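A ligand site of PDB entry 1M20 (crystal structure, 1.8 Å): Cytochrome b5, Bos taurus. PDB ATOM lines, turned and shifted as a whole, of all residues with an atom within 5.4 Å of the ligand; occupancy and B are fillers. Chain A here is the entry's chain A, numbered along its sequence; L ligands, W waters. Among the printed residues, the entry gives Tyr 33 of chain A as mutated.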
ATOM      1  N   LEU A  21      16.560  -6.925  13.111  1.00  0.00           N
ATOM      2  CA  LEU A  21      16.389  -6.550  14.499  1.00  0.00           C
ATOM      3  C   LEU A  21      16.524  -5.043  14.604  1.00  0.00           C
ATOM      4  O   LEU A  21      17.042  -4.380  13.692  1.00  0.00           O
ATOM      5  CB  LEU A  21      17.369  -7.285  15.416  1.00  0.00           C
ATOM      6  CG  LEU A  21      18.876  -7.324  15.186  1.00  0.00           C
ATOM      7  CD1 LEU A  21      19.505  -5.975  15.501  1.00  0.00           C
ATOM      8  CD2 LEU A  21      19.461  -8.406  16.091  1.00  0.00           C
ATOM      9  N   LEU A  23      17.824  -1.597  16.679  1.00  0.00           N
ATOM     10  CA  LEU A  23      18.774  -1.073  17.652  1.00  0.00           C
ATOM     11  C   LEU A  23      18.642   0.444  17.590  1.00  0.00           C
ATOM     12  O   LEU A  23      18.854   1.037  16.544  1.00  0.00           O
ATOM     13  CB  LEU A  23      20.214  -1.462  17.311  1.00  0.00           C
ATOM     14  CG  LEU A  23      20.600  -2.946  17.370  1.00  0.00           C
ATOM     15  CD1 LEU A  23      22.078  -3.067  17.034  1.00  0.00           C
ATOM     16  CD2 LEU A  23      20.313  -3.534  18.734  1.00  0.00           C
ATOM     17  N   TYR A  28      18.091  -3.192  11.272  1.00  0.00           N
ATOM     18  CA  TYR A  28      19.277  -3.825  10.722  1.00  0.00           C
ATOM     19  C   TYR A  28      18.932  -5.177  10.121  1.00  0.00           C
ATOM     20  O   TYR A  28      18.215  -5.962  10.728  1.00  0.00           O
ATOM     21  CB  TYR A  28      20.329  -4.050  11.800  1.00  0.00           C
ATOM     22  CG  TYR A  28      20.866  -2.794  12.441  1.00  0.00           C
ATOM     23  CD1 TYR A  28      20.085  -2.058  13.330  1.00  0.00           C
ATOM     24  CD2 TYR A  28      22.144  -2.331  12.145  1.00  0.00           C
ATOM     25  CE1 TYR A  28      20.554  -0.882  13.896  1.00  0.00           C
ATOM     26  CE2 TYR A  28      22.632  -1.145  12.714  1.00  0.00           C
ATOM     27  CZ  TYR A  28      21.819  -0.426  13.584  1.00  0.00           C
ATOM     28  OH  TYR A  28      22.267   0.751  14.124  1.00  0.00           O
ATOM     29  N   LEU A  30      20.554  -8.403   9.477  1.00  0.00           N
ATOM     30  CA  LEU A  30      21.764  -9.150   9.802  1.00  0.00           C
ATOM     31  C   LEU A  30      21.812 -10.563   9.206  1.00  0.00           C
ATOM     32  O   LEU A  30      22.638 -11.380   9.625  1.00  0.00           O
ATOM     33  CB  LEU A  30      21.912  -9.255  11.319  1.00  0.00           C
ATOM     34  CG  LEU A  30      21.950  -7.927  12.077  1.00  0.00           C
ATOM     35  CD1 LEU A  30      22.118  -8.207  13.567  1.00  0.00           C
ATOM     36  CD2 LEU A  30      23.087  -7.065  11.553  1.00  0.00           C
ATOM     37  N   TYR A  33      25.169 -11.621   8.193  1.00  0.00           N
ATOM     38  CA  TYR A  33      26.196 -11.374   9.203  1.00  0.00           C
ATOM     39  C   TYR A  33      26.212 -12.425  10.310  1.00  0.00           C
ATOM     40  O   TYR A  33      27.199 -12.552  11.041  1.00  0.00           O
ATOM     41  CB  TYR A  33      25.978  -9.993   9.810  1.00  0.00           C
ATOM     42  CG  TYR A  33      27.021  -9.613  10.829  1.00  0.00           C
ATOM     43  CD1 TYR A  33      26.671  -9.330  12.144  1.00  0.00           C
ATOM     44  CD2 TYR A  33      28.370  -9.557  10.471  1.00  0.00           C
ATOM     45  CE1 TYR A  33      27.634  -8.994  13.083  1.00  0.00           C
ATOM     46  CE2 TYR A  33      29.345  -9.226  11.407  1.00  0.00           C
ATOM     47  CZ  TYR A  33      28.969  -8.945  12.709  1.00  0.00           C
ATOM     48  OH  TYR A  33      29.915  -8.634  13.642  1.00  0.00           O
ATOM     49  N   HIS A  37      29.524 -12.821  13.001  1.00  0.00           N
ATOM     50  CA  HIS A  37      29.440 -12.176  14.313  1.00  0.00           C
ATOM     51  C   HIS A  37      30.316 -12.858  15.364  1.00  0.00           C
ATOM     52  O   HIS A  37      30.109 -14.021  15.686  1.00  0.00           O
ATOM     53  CB  HIS A  37      27.989 -12.182  14.781  1.00  0.00           C
ATOM     54  CG  HIS A  37      27.780 -11.501  16.093  1.00  0.00           C
ATOM     55  ND1 HIS A  37      27.035 -12.036  17.125  1.00  0.00           N
ATOM     56  CD2 HIS A  37      28.194 -10.284  16.532  1.00  0.00           C
ATOM     57  CE1 HIS A  37      27.013 -11.145  18.120  1.00  0.00           C
ATOM     58  NE2 HIS A  37      27.706 -10.062  17.800  1.00  0.00           N
ATOM     59  N   PRO A  38      31.304 -12.133  15.918  1.00  0.00           N
ATOM     60  CA  PRO A  38      32.197 -12.685  16.953  1.00  0.00           C
ATOM     61  C   PRO A  38      31.438 -13.244  18.156  1.00  0.00           C
ATOM     62  O   PRO A  38      31.903 -14.167  18.815  1.00  0.00           O
ATOM     63  CB  PRO A  38      33.070 -11.491  17.325  1.00  0.00           C
ATOM     64  CG  PRO A  38      33.165 -10.744  16.025  1.00  0.00           C
ATOM     65  CD  PRO A  38      31.736 -10.780  15.530  1.00  0.00           C
ATOM     66  N   GLY A  39      30.271 -12.677  18.427  1.00  0.00           N
ATOM     67  CA  GLY A  39      29.469 -13.130  19.558  1.00  0.00           C
ATOM     68  C   GLY A  39      28.599 -14.342  19.254  1.00  0.00           C
ATOM     69  O   GLY A  39      27.855 -14.806  20.129  1.00  0.00           O
ATOM     70  N   VAL A  43      22.904 -15.672  19.666  1.00  0.00           N
ATOM     71  CA  VAL A  43      22.466 -14.473  20.374  1.00  0.00           C
ATOM     72  C   VAL A  43      21.709 -13.507  19.457  1.00  0.00           C
ATOM     73  O   VAL A  43      20.885 -12.714  19.917  1.00  0.00           O
ATOM     74  CB  VAL A  43      23.672 -13.739  21.029  1.00  0.00           C
ATOM     75  CG1 VAL A  43      24.444 -12.957  19.984  1.00  0.00           C
ATOM     76  CG2 VAL A  43      23.181 -12.843  22.139  1.00  0.00           C
ATOM     77  N   LEU A  44      21.975 -13.575  18.157  1.00  0.00           N
ATOM     78  CA  LEU A  44      21.287 -12.701  17.209  1.00  0.00           C
ATOM     79  C   LEU A  44      19.917 -13.276  16.861  1.00  0.00           C
ATOM     80  O   LEU A  44      18.914 -12.563  16.877  1.00  0.00           O
ATOM     81  CB  LEU A  44      22.133 -12.525  15.949  1.00  0.00           C
ATOM     82  CG  LEU A  44      23.489 -11.851  16.165  1.00  0.00           C
ATOM     83  CD1 LEU A  44      24.226 -11.694  14.858  1.00  0.00           C
ATOM     84  CD2 LEU A  44      23.266 -10.492  16.811  1.00  0.00           C
ATOM     85  N   GLN A  47      17.026 -12.599  19.251  1.00  0.00           N
ATOM     86  CA  GLN A  47      16.445 -11.262  19.258  1.00  0.00           C
ATOM     87  C   GLN A  47      15.775 -10.890  17.936  1.00  0.00           C
ATOM     88  O   GLN A  47      15.150  -9.835  17.836  1.00  0.00           O
ATOM     89  CB  GLN A  47      17.533 -10.222  19.562  1.00  0.00           C
ATOM     90  CG  GLN A  47      18.210 -10.394  20.921  1.00  0.00           C
ATOM     91  CD  GLN A  47      17.262 -10.163  22.077  1.00  0.00           C
ATOM     92  OE1 GLN A  47      16.525  -9.173  22.108  1.00  0.00           O
ATOM     93  NE2 GLN A  47      17.277 -11.074  23.043  1.00  0.00           N
ATOM     94  N   ALA A  52      16.518  -5.104  20.177  1.00  0.00           N
ATOM     95  CA  ALA A  52      17.619  -5.702  20.929  1.00  0.00           C
ATOM     96  C   ALA A  52      18.577  -4.654  21.479  1.00  0.00           C
ATOM     97  O   ALA A  52      19.720  -4.980  21.832  1.00  0.00           O
ATOM     98  CB  ALA A  52      18.371  -6.675  20.031  1.00  0.00           C
ATOM     99  N   ASN A  55      20.098  -5.370  25.105  1.00  0.00           N
ATOM    100  CA  ASN A  55      21.047  -6.484  25.075  1.00  0.00           C
ATOM    101  C   ASN A  55      22.342  -6.083  24.388  1.00  0.00           C
ATOM    102  O   ASN A  55      23.431  -6.481  24.802  1.00  0.00           O
ATOM    103  CB  ASN A  55      20.434  -7.681  24.350  1.00  0.00           C
ATOM    104  CG  ASN A  55      19.004  -7.950  24.761  1.00  0.00           C
ATOM    105  OD1 ASN A  55      18.075  -7.451  24.135  1.00  0.00           O
ATOM    106  ND2 ASN A  55      18.836  -8.721  25.823  1.00  0.00           N
ATOM    107  N   PHE A  56      22.205  -5.288  23.329  1.00  0.00           N
ATOM    108  CA  PHE A  56      23.340  -4.808  22.565  1.00  0.00           C
ATOM    109  C   PHE A  56      24.242  -3.917  23.424  1.00  0.00           C
ATOM    110  O   PHE A  56      25.465  -4.024  23.382  1.00  0.00           O
ATOM    111  CB  PHE A  56      22.847  -4.029  21.347  1.00  0.00           C
ATOM    112  CG  PHE A  56      23.943  -3.481  20.486  1.00  0.00           C
ATOM    113  CD1 PHE A  56      24.648  -4.313  19.610  1.00  0.00           C
ATOM    114  CD2 PHE A  56      24.269  -2.133  20.528  1.00  0.00           C
ATOM    115  CE1 PHE A  56      25.661  -3.796  18.792  1.00  0.00           C
ATOM    116  CE2 PHE A  56      25.277  -1.610  19.716  1.00  0.00           C
ATOM    117  CZ  PHE A  56      25.968  -2.446  18.849  1.00  0.00           C
ATOM    118  N   VAL A  59      26.235  -5.634  26.624  1.00  0.00           N
ATOM    119  CA  VAL A  59      27.511  -6.291  26.356  1.00  0.00           C
ATOM    120  C   VAL A  59      28.608  -5.265  26.110  1.00  0.00           C
ATOM    121  O   VAL A  59      29.795  -5.589  26.189  1.00  0.00           O
ATOM    122  CB  VAL A  59      27.401  -7.234  25.135  1.00  0.00           C
ATOM    123  CG1 VAL A  59      26.386  -8.330  25.409  1.00  0.00           C
ATOM    124  CG2 VAL A  59      26.985  -6.455  23.920  1.00  0.00           C
ATOM    125  N   GLY A  60      28.214  -4.027  25.819  1.00  0.00           N
ATOM    126  CA  GLY A  60      29.181  -2.957  25.605  1.00  0.00           C
ATOM    127  C   GLY A  60      30.055  -3.079  24.371  1.00  0.00           C
ATOM    128  O   GLY A  60      31.291  -3.144  24.480  1.00  0.00           O
ATOM    129  N   HIS A  61      29.440  -3.079  23.196  1.00  0.00           N
ATOM    130  CA  HIS A  61      30.168  -3.186  21.939  1.00  0.00           C
ATOM    131  C   HIS A  61      31.179  -2.070  21.716  1.00  0.00           C
ATOM    132  O   HIS A  61      30.939  -0.921  22.071  1.00  0.00           O
ATOM    133  CB  HIS A  61      29.205  -3.210  20.751  1.00  0.00           C
ATOM    134  CG  HIS A  61      28.516  -4.522  20.577  1.00  0.00           C
ATOM    135  ND1 HIS A  61      27.457  -4.958  21.338  1.00  0.00           N
ATOM    136  CD2 HIS A  61      28.796  -5.543  19.722  1.00  0.00           C
ATOM    137  CE1 HIS A  61      27.137  -6.194  20.937  1.00  0.00           C
ATOM    138  NE2 HIS A  61      27.927  -6.584  19.956  1.00  0.00           N
ATOM    139  N   SER A  62      32.301  -2.442  21.107  1.00  0.00           N
ATOM    140  CA  SER A  62      33.382  -1.508  20.823  1.00  0.00           C
ATOM    141  C   SER A  62      33.014  -0.528  19.721  1.00  0.00           C
ATOM    142  O   SER A  62      32.027  -0.710  19.008  1.00  0.00           O
ATOM    143  CB  SER A  62      34.625  -2.281  20.391  1.00  0.00           C
ATOM    144  OG  SER A  62      34.412  -2.916  19.137  1.00  0.00           O
ATOM    145  N   ALA A  65      32.824  -2.145  16.285  1.00  0.00           N
ATOM    146  CA  ALA A  65      31.619  -2.929  16.055  1.00  0.00           C
ATOM    147  C   ALA A  65      30.464  -2.002  15.672  1.00  0.00           C
ATOM    148  O   ALA A  65      29.696  -2.299  14.760  1.00  0.00           O
ATOM    149  CB  ALA A  65      31.266  -3.719  17.298  1.00  0.00           C
ATOM    150  N   LEU A  68      30.931  -0.714  12.174  1.00  0.00           N
ATOM    151  CA  LEU A  68      30.596  -1.755  11.209  1.00  0.00           C
ATOM    152  C   LEU A  68      29.091  -1.963  11.090  1.00  0.00           C
ATOM    153  O   LEU A  68      28.581  -2.161   9.994  1.00  0.00           O
ATOM    154  CB  LEU A  68      31.263  -3.070  11.598  1.00  0.00           C
ATOM    155  CG  LEU A  68      30.842  -4.309  10.807  1.00  0.00           C
ATOM    156  CD1 LEU A  68      31.195  -4.148   9.325  1.00  0.00           C
ATOM    157  CD2 LEU A  68      31.529  -5.544  11.392  1.00  0.00           C
ATOM    158  N   SER A  69      28.379  -1.917  12.212  1.00  0.00           N
ATOM    159  CA  SER A  69      26.933  -2.140  12.205  1.00  0.00           C
ATOM    160  C   SER A  69      26.165  -1.229  11.253  1.00  0.00           C
ATOM    161  O   SER A  69      25.135  -1.616  10.717  1.00  0.00           O
ATOM    162  CB  SER A  69      26.368  -1.979  13.622  1.00  0.00           C
ATOM    163  OG  SER A  69      26.313  -0.620  14.011  1.00  0.00           O
ATOM    164  N   PHE A  72      24.723  -2.352   7.863  1.00  0.00           N
ATOM    165  CA  PHE A  72      23.541  -3.211   7.809  1.00  0.00           C
ATOM    166  C   PHE A  72      22.200  -2.509   7.995  1.00  0.00           C
ATOM    167  O   PHE A  72      21.148  -3.155   8.021  1.00  0.00           O
ATOM    168  CB  PHE A  72      23.676  -4.339   8.847  1.00  0.00           C
ATOM    169  CG  PHE A  72      24.911  -5.190   8.655  1.00  0.00           C
ATOM    170  CD1 PHE A  72      25.086  -5.947   7.500  1.00  0.00           C
ATOM    171  CD2 PHE A  72      25.917  -5.202   9.623  1.00  0.00           C
ATOM    172  CE1 PHE A  72      26.243  -6.720   7.317  1.00  0.00           C
ATOM    173  CE2 PHE A  72      27.070  -5.969   9.447  1.00  0.00           C
ATOM    174  CZ  PHE A  72      27.232  -6.721   8.295  1.00  0.00           C
HETATM  175  C1  LIG L   1      30.691  -9.318  20.333  1.00  0.00           C
HETATM  176  C2  LIG L   1      29.680  -6.846  16.305  1.00  0.00           C
HETATM  177  C3  LIG L   1      24.968  -7.112  17.418  1.00  0.00           C
HETATM  178  C4  LIG L   1      25.963  -9.791  21.315  1.00  0.00           C
HETATM  179  C5  LIG L   1      30.817  -8.561  19.177  1.00  0.00           C
HETATM  180  C6  LIG L   1      32.076  -8.143  18.606  1.00  0.00           C
HETATM  181  C7  LIG L   1      31.792  -7.510  17.447  1.00  0.00           C
HETATM  182  C8  LIG L   1      30.346  -7.495  17.323  1.00  0.00           C
HETATM  183  C9  LIG L   1      32.769  -6.915  16.432  1.00  0.00           C
HETATM  184  C10 LIG L   1      33.461  -8.293  19.209  1.00  0.00           C
HETATM  185  C11 LIG L   1      33.707  -7.430  20.440  1.00  0.00           C
HETATM  186  C12 LIG L   1      33.496  -5.949  20.158  1.00  0.00           C
HETATM  187  O1  LIG L   1      34.089  -5.439  19.193  1.00  0.00           O
HETATM  188  O2  LIG L   1      32.744  -5.309  20.916  1.00  0.00           O
HETATM  189  C13 LIG L   1      28.288  -6.717  16.252  1.00  0.00           C
HETATM  190  C14 LIG L   1      27.570  -6.042  15.200  1.00  0.00           C
HETATM  191  C15 LIG L   1      26.243  -6.150  15.499  1.00  0.00           C
HETATM  192  C16 LIG L   1      26.158  -6.846  16.768  1.00  0.00           C
HETATM  193  C17 LIG L   1      28.188  -5.380  13.966  1.00  0.00           C
HETATM  194  C18 LIG L   1      25.186  -5.825  14.643  1.00  0.00           C
HETATM  195  C19 LIG L   1      24.399  -4.700  14.821  1.00  0.00           C
HETATM  196  C20 LIG L   1      24.842  -7.835  18.590  1.00  0.00           C
HETATM  197  C21 LIG L   1      23.582  -8.015  19.301  1.00  0.00           C
HETATM  198  C22 LIG L   1      23.841  -8.799  20.379  1.00  0.00           C
HETATM  199  C23 LIG L   1      25.272  -9.087  20.338  1.00  0.00           C
HETATM  200  C24 LIG L   1      22.232  -7.438  18.884  1.00  0.00           C
HETATM  201  C25 LIG L   1      22.951  -9.206  21.361  1.00  0.00           C
HETATM  202  C26 LIG L   1      21.637  -9.670  21.154  1.00  0.00           C
HETATM  203  C27 LIG L   1      27.353  -9.898  21.365  1.00  0.00           C
HETATM  204  C28 LIG L   1      28.070 -10.660  22.371  1.00  0.00           C
HETATM  205  C29 LIG L   1      29.382 -10.544  22.098  1.00  0.00           C
HETATM  206  C30 LIG L   1      29.493  -9.686  20.929  1.00  0.00           C
HETATM  207  C31 LIG L   1      27.453 -11.459  23.514  1.00  0.00           C
HETATM  208  C32 LIG L   1      30.511 -11.249  22.860  1.00  0.00           C
HETATM  209  C33 LIG L   1      31.293 -10.342  23.804  1.00  0.00           C
HETATM  210  C34 LIG L   1      32.375 -11.090  24.557  1.00  0.00           C
HETATM  211  O3  LIG L   1      33.260 -11.679  23.905  1.00  0.00           O
HETATM  212  O4  LIG L   1      32.341 -11.096  25.808  1.00  0.00           O
HETATM  213  N1  LIG L   1      29.750  -8.121  18.409  1.00  0.00           N
HETATM  214  N2  LIG L   1      27.420  -7.225  17.210  1.00  0.00           N
HETATM  215  N3  LIG L   1      25.894  -8.459  19.265  1.00  0.00           N
HETATM  216  N4  LIG L   1      28.234  -9.324  20.461  1.00  0.00           N
HETATM  217 FE1  LIG L   1      27.834  -8.310  18.818  1.00  0.00          FE
HETATM  218  O   HOH W   1      34.421 -10.663  21.588  1.00  0.00           O
HETATM  219  O   HOH W   2      28.303 -14.783  23.012  1.00  0.00           O
HETATM  220  O   HOH W   3      33.570  -8.167  24.483  1.00  0.00           O
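Residues that only touch the ligand: Leu 23 (3.6 Å), Leu 30 (3.9 Å), Tyr 33 (3.2 Å), Pro 38 (3.7 Å), Gly 39 (3.6 Å), Val 43 (3.4 Å), Leu 44 (3.5 Å), Gln 47 (3.5 Å), Asn 55 (3.95 Å), Phe 56 (3.6 Å), Val 59 (3.8 Å), Ala 65 (3.5 Å) and Ser 69 (3.6 Å). Hydrophobic or aromatic side chains that line the ligand: Leu 23, Leu 30, Tyr 33, His 37, Pro 38, Val 43, Leu 44, Phe 56, Val 59, His 61 and Ala 65. 16 residues have an atom within 4 Å of the ligand: Leu 23, Leu 30, Tyr 33, His 37, Pro 38, Gly 39, Val 43, Leu 44, Gln 47, Asn 55, Phe 56, Val 59, His 61, Ser 62, Ala 65 and Ser 69.
A ring nitrogen (ND1) of His 61 sits at hydrogen-bond distance from the backbone carbonyl oxygen of Phe 56 (3.0 Å). N of Ala 65 sits at hydrogen-bond distance from OG of Ser 62, 3.4 Å away. The side-chain amide oxygen of Gln 47 sits close to the side-chain amide oxygen of Asn 55, at 3.1 Å.
An oxygen (O2) of the ligand sits at hydrogen-bond distance from the backbone NH (N) of Ser 62 (2.9 Å). A ring nitrogen (NE2) of His 61 binds an iron atom (FE1) of the ligand, at 2.1 Å. NE2 of His 37 is bound to FE1 of the ligand (2.0 Å). The side-chain hydroxyl (OG) of Ser 62 sits at hydrogen-bond distance from an oxygen (O1) of the ligand (2.5 Å).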
